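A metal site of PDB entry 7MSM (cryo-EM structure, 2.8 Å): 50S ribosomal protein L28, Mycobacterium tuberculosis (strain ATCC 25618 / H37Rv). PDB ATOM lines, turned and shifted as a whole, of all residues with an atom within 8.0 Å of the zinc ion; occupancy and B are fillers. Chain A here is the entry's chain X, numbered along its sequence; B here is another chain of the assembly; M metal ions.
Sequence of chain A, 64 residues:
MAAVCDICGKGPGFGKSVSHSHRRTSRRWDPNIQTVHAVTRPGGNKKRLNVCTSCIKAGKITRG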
ATOM      1  N   VAL A   4     -19.774  24.753  -8.847  1.00  0.00           N
ATOM      2  CA  VAL A   4     -21.099  24.490  -9.388  1.00  0.00           C
ATOM      3  C   VAL A   4     -22.026  24.204  -8.224  1.00  0.00           C
ATOM      4  O   VAL A   4     -21.768  23.305  -7.428  1.00  0.00           O
ATOM      5  CB  VAL A   4     -21.097  23.322 -10.382  1.00  0.00           C
ATOM      6  CG1 VAL A   4     -22.494  23.030 -10.843  1.00  0.00           C
ATOM      7  CG2 VAL A   4     -20.231  23.637 -11.572  1.00  0.00           C
ATOM      8  N   CYS A   5     -23.109  24.984  -8.122  1.00  0.00           N
ATOM      9  CA  CYS A   5     -24.057  24.809  -7.036  1.00  0.00           C
ATOM     10  C   CYS A   5     -24.875  23.549  -7.264  1.00  0.00           C
ATOM     11  O   CYS A   5     -25.376  23.298  -8.359  1.00  0.00           O
ATOM     12  CB  CYS A   5     -24.980  26.014  -6.947  1.00  0.00           C
ATOM     13  SG  CYS A   5     -26.158  26.002  -5.575  1.00  0.00           S
ATOM     14  N   ASP A   6     -25.041  22.760  -6.213  1.00  0.00           N
ATOM     15  CA  ASP A   6     -25.724  21.485  -6.319  1.00  0.00           C
ATOM     16  C   ASP A   6     -27.237  21.594  -6.206  1.00  0.00           C
ATOM     17  O   ASP A   6     -27.901  20.560  -6.124  1.00  0.00           O
ATOM     18  CB  ASP A   6     -25.224  20.516  -5.260  1.00  0.00           C
ATOM     19  CG  ASP A   6     -23.845  20.006  -5.561  1.00  0.00           C
ATOM     20  OD1 ASP A   6     -23.489  19.929  -6.743  1.00  0.00           O
ATOM     21  OD2 ASP A   6     -23.120  19.656  -4.611  1.00  0.00           O
ATOM     22  N   ILE A   7     -27.808  22.799  -6.213  1.00  0.00           N
ATOM     23  CA  ILE A   7     -29.261  22.935  -6.173  1.00  0.00           C
ATOM     24  C   ILE A   7     -29.759  23.705  -7.378  1.00  0.00           C
ATOM     25  O   ILE A   7     -30.591  23.203  -8.137  1.00  0.00           O
ATOM     26  CB  ILE A   7     -29.717  23.599  -4.863  1.00  0.00           C
ATOM     27  CG1 ILE A   7     -29.492  22.657  -3.694  1.00  0.00           C
ATOM     28  CG2 ILE A   7     -31.178  23.994  -4.935  1.00  0.00           C
ATOM     29  CD1 ILE A   7     -29.793  23.264  -2.397  1.00  0.00           C
ATOM     30  N   CYS A   8     -29.250  24.914  -7.592  1.00  0.00           N
ATOM     31  CA  CYS A   8     -29.721  25.747  -8.688  1.00  0.00           C
ATOM     32  C   CYS A   8     -28.839  25.677  -9.914  1.00  0.00           C
ATOM     33  O   CYS A   8     -29.162  26.294 -10.928  1.00  0.00           O
ATOM     34  CB  CYS A   8     -29.859  27.205  -8.237  1.00  0.00           C
ATOM     35  SG  CYS A   8     -28.327  28.044  -7.856  1.00  0.00           S
ATOM     36  N   GLY A   9     -27.736  24.927  -9.860  1.00  0.00           N
ATOM     37  CA  GLY A   9     -26.934  24.714 -11.041  1.00  0.00           C
ATOM     38  C   GLY A   9     -26.117  25.898 -11.471  1.00  0.00           C
ATOM     39  O   GLY A   9     -25.651  25.947 -12.608  1.00  0.00           O
ATOM     40  N   LYS A  10     -25.928  26.867 -10.579  1.00  0.00           N
ATOM     41  CA  LYS A  10     -25.231  28.093 -10.925  1.00  0.00           C
ATOM     42  C   LYS A  10     -23.744  27.836 -11.061  1.00  0.00           C
ATOM     43  O   LYS A  10     -23.145  27.175 -10.213  1.00  0.00           O
ATOM     44  CB  LYS A  10     -25.519  29.154  -9.869  1.00  0.00           C
ATOM     45  CG  LYS A  10     -24.912  30.499 -10.113  1.00  0.00           C
ATOM     46  CD  LYS A  10     -25.561  31.548  -9.227  1.00  0.00           C
ATOM     47  CE  LYS A  10     -25.161  31.454  -7.789  1.00  0.00           C
ATOM     48  NZ  LYS A  10     -25.801  32.551  -7.032  1.00  0.00           N
ATOM     49  N   PRO A  31     -19.074  31.298  -8.370  1.00  0.00           N
ATOM     50  CA  PRO A  31     -20.092  31.562  -7.352  1.00  0.00           C
ATOM     51  C   PRO A  31     -19.577  31.209  -5.971  1.00  0.00           C
ATOM     52  O   PRO A  31     -18.712  30.359  -5.809  1.00  0.00           O
ATOM     53  CB  PRO A  31     -21.246  30.666  -7.775  1.00  0.00           C
ATOM     54  CG  PRO A  31     -20.618  29.596  -8.512  1.00  0.00           C
ATOM     55  CD  PRO A  31     -19.457  30.171  -9.221  1.00  0.00           C
ATOM     56  N   ASN A  32     -20.103  31.922  -4.980  1.00  0.00           N
ATOM     57  CA  ASN A  32     -19.635  31.764  -3.613  1.00  0.00           C
ATOM     58  C   ASN A  32     -20.204  30.455  -3.072  1.00  0.00           C
ATOM     59  O   ASN A  32     -21.217  30.416  -2.378  1.00  0.00           O
ATOM     60  CB  ASN A  32     -20.045  32.960  -2.768  1.00  0.00           C
ATOM     61  CG  ASN A  32     -19.352  33.008  -1.439  1.00  0.00           C
ATOM     62  OD1 ASN A  32     -18.561  32.145  -1.100  1.00  0.00           O
ATOM     63  ND2 ASN A  32     -19.655  34.035  -0.653  1.00  0.00           N
ATOM     64  N   ILE A  33     -19.528  29.369  -3.409  1.00  0.00           N
ATOM     65  CA  ILE A  33     -19.961  28.027  -3.041  1.00  0.00           C
ATOM     66  C   ILE A  33     -19.423  27.720  -1.659  1.00  0.00           C
ATOM     67  O   ILE A  33     -18.213  27.724  -1.430  1.00  0.00           O
ATOM     68  CB  ILE A  33     -19.487  26.996  -4.060  1.00  0.00           C
ATOM     69  CG1 ILE A  33     -20.039  27.320  -5.444  1.00  0.00           C
ATOM     70  CG2 ILE A  33     -19.924  25.630  -3.632  1.00  0.00           C
ATOM     71  CD1 ILE A  33     -21.513  27.323  -5.519  1.00  0.00           C
ATOM     72  N   ASN A  50     -22.695  21.069  -1.811  1.00  0.00           N
ATOM     73  CA  ASN A  50     -22.000  22.297  -2.188  1.00  0.00           C
ATOM     74  C   ASN A  50     -23.050  23.253  -2.718  1.00  0.00           C
ATOM     75  O   ASN A  50     -23.538  23.078  -3.833  1.00  0.00           O
ATOM     76  CB  ASN A  50     -20.930  22.046  -3.242  1.00  0.00           C
ATOM     77  CG  ASN A  50     -19.769  21.238  -2.727  1.00  0.00           C
ATOM     78  OD1 ASN A  50     -19.343  21.377  -1.592  1.00  0.00           O
ATOM     79  ND2 ASN A  50     -19.232  20.389  -3.593  1.00  0.00           N
ATOM     80  N   VAL A  51     -23.402  24.270  -1.937  1.00  0.00           N
ATOM     81  CA  VAL A  51     -24.442  25.213  -2.319  1.00  0.00           C
ATOM     82  C   VAL A  51     -23.869  26.614  -2.357  1.00  0.00           C
ATOM     83  O   VAL A  51     -22.836  26.912  -1.761  1.00  0.00           O
ATOM     84  CB  VAL A  51     -25.642  25.151  -1.356  1.00  0.00           C
ATOM     85  CG1 VAL A  51     -26.256  23.785  -1.379  1.00  0.00           C
ATOM     86  CG2 VAL A  51     -25.176  25.424   0.003  1.00  0.00           C
ATOM     87  N   CYS A  52     -24.539  27.490  -3.088  1.00  0.00           N
ATOM     88  CA  CYS A  52     -24.122  28.878  -3.163  1.00  0.00           C
ATOM     89  C   CYS A  52     -24.754  29.674  -2.026  1.00  0.00           C
ATOM     90  O   CYS A  52     -25.665  29.206  -1.338  1.00  0.00           O
ATOM     91  CB  CYS A  52     -24.501  29.495  -4.506  1.00  0.00           C
ATOM     92  SG  CYS A  52     -26.251  29.620  -4.806  1.00  0.00           S
ATOM     93  N   THR A  53     -24.241  30.876  -1.810  1.00  0.00           N
ATOM     94  CA  THR A  53     -24.700  31.681  -0.685  1.00  0.00           C
ATOM     95  C   THR A  53     -26.052  32.312  -0.920  1.00  0.00           C
ATOM     96  O   THR A  53     -26.760  32.616   0.037  1.00  0.00           O
ATOM     97  CB  THR A  53     -23.702  32.772  -0.371  1.00  0.00           C
ATOM     98  OG1 THR A  53     -23.430  33.518  -1.562  1.00  0.00           O
ATOM     99  CG2 THR A  53     -22.440  32.181   0.156  1.00  0.00           C
ATOM    100  N   SER A  54     -26.435  32.515  -2.183  1.00  0.00           N
ATOM    101  CA  SER A  54     -27.754  33.063  -2.468  1.00  0.00           C
ATOM    102  C   SER A  54     -28.870  32.066  -2.232  1.00  0.00           C
ATOM    103  O   SER A  54     -30.037  32.472  -2.226  1.00  0.00           O
ATOM    104  CB  SER A  54     -27.782  33.568  -3.900  1.00  0.00           C
ATOM    105  OG  SER A  54     -27.627  32.492  -4.797  1.00  0.00           O
ATOM    106  N   CYS A  55     -28.561  30.793  -2.026  1.00  0.00           N
ATOM    107  CA  CYS A  55     -29.545  29.799  -1.635  1.00  0.00           C
ATOM    108  C   CYS A  55     -29.507  29.479  -0.150  1.00  0.00           C
ATOM    109  O   CYS A  55     -30.485  28.931   0.364  1.00  0.00           O
ATOM    110  CB  CYS A  55     -29.352  28.512  -2.439  1.00  0.00           C
ATOM    111  SG  CYS A  55     -29.721  28.677  -4.195  1.00  0.00           S
ATOM    112  N   ILE A  56     -28.420  29.774   0.546  1.00  0.00           N
ATOM    113  CA  ILE A  56     -28.426  29.661   1.998  1.00  0.00           C
ATOM    114  C   ILE A  56     -29.132  30.873   2.581  1.00  0.00           C
ATOM    115  O   ILE A  56     -29.735  30.796   3.664  1.00  0.00           O
ATOM    116  CB  ILE A  56     -26.999  29.536   2.539  1.00  0.00           C
ATOM    117  CG1 ILE A  56     -26.253  28.420   1.831  1.00  0.00           C
ATOM    118  CG2 ILE A  56     -26.982  29.161   3.991  1.00  0.00           C
ATOM    119  CD1 ILE A  56     -24.798  28.424   2.132  1.00  0.00           C
ATOM    120  N   LYS A  60     -33.539  27.453   1.029  1.00  0.00           N
ATOM    121  CA  LYS A  60     -33.429  26.283   0.171  1.00  0.00           C
ATOM    122  C   LYS A  60     -32.853  25.070   0.881  1.00  0.00           C
ATOM    123  O   LYS A  60     -33.047  23.949   0.411  1.00  0.00           O
ATOM    124  CB  LYS A  60     -32.576  26.606  -1.053  1.00  0.00           C
ATOM    125  CG  LYS A  60     -33.050  27.778  -1.925  1.00  0.00           C
ATOM    126  CD  LYS A  60     -34.243  27.457  -2.811  1.00  0.00           C
ATOM    127  CE  LYS A  60     -35.546  28.005  -2.265  1.00  0.00           C
ATOM    128  NZ  LYS A  60     -36.678  27.781  -3.207  1.00  0.00           N
ATOM    129  P     U B 486     -22.568  34.626  -6.795  1.00  0.00           P
ATOM    130  OP1   U B 486     -22.396  33.499  -5.881  1.00  0.00           O
ATOM    131  OP2   U B 486     -23.931  35.045  -7.160  1.00  0.00           O
ATOM    132  O5'   U B 486     -21.811  35.866  -6.158  1.00  0.00           O
ATOM    133  C5'   U B 486     -20.563  35.717  -5.505  1.00  0.00           C
ATOM    134  C4'   U B 486     -20.134  37.007  -4.874  1.00  0.00           C
ATOM    135  O4'   U B 486     -19.991  38.014  -5.898  1.00  0.00           O
ATOM    136  C3'   U B 486     -21.121  37.618  -3.914  1.00  0.00           C
ATOM    137  O3'   U B 486     -21.066  37.054  -2.628  1.00  0.00           O
ATOM    138  C2'   U B 486     -20.747  39.087  -3.941  1.00  0.00           C
ATOM    139  O2'   U B 486     -19.602  39.309  -3.142  1.00  0.00           O
ATOM    140  C1'   U B 486     -20.357  39.265  -5.400  1.00  0.00           C
ATOM    141  N1    U B 486     -21.455  39.814  -6.217  1.00  0.00           N
ATOM    142  C2    U B 486     -21.632  41.169  -6.218  1.00  0.00           C
ATOM    143  O2    U B 486     -20.942  41.931  -5.558  1.00  0.00           O
ATOM    144  N3    U B 486     -22.634  41.624  -7.008  1.00  0.00           N
ATOM    145  C4    U B 486     -23.474  40.885  -7.783  1.00  0.00           C
ATOM    146  O4    U B 486     -24.342  41.437  -8.450  1.00  0.00           O
ATOM    147  C5    U B 486     -23.226  39.492  -7.745  1.00  0.00           C
ATOM    148  C6    U B 486     -22.241  39.035  -7.003  1.00  0.00           C
HETATM  149 ZN    ZN M   1     -27.793  27.869  -5.498  1.00  0.00          ZN
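The side-chain hydroxyl (OG) of Ser 54 lies close to the side-chain sulfur (SG) of Cys 52.
The side-chain amino group of Lys 10 lies close to the side-chain sulfur of Cys 52, 3.7 Å away.
The backbone carbonyl oxygen (O) of Cys 55 sits close to the backbone NH (N) of Lys 60 (3.5 Å).
SG of Cys 5 lies close to N of Ile 7 (3.7 Å).
The backbone NH (N) of Cys 5 sits at hydrogen-bond distance from the backbone carbonyl oxygen (O) of Lys 10 (3.0 Å).
Within 4 Å of the zinc ion: Cys 5, Cys 8, Cys 52 and Cys 55.
The nearest printed residue that does not touch the zinc ion is Ser 54 (4.7 Å).
The zinc ion is bound by SG of Cys 8 (2.4 Å), SG of Cys 52 (2.4 Å), SG of Cys 55 (2.5 Å) and SG of Cys 5 (2.5 Å).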
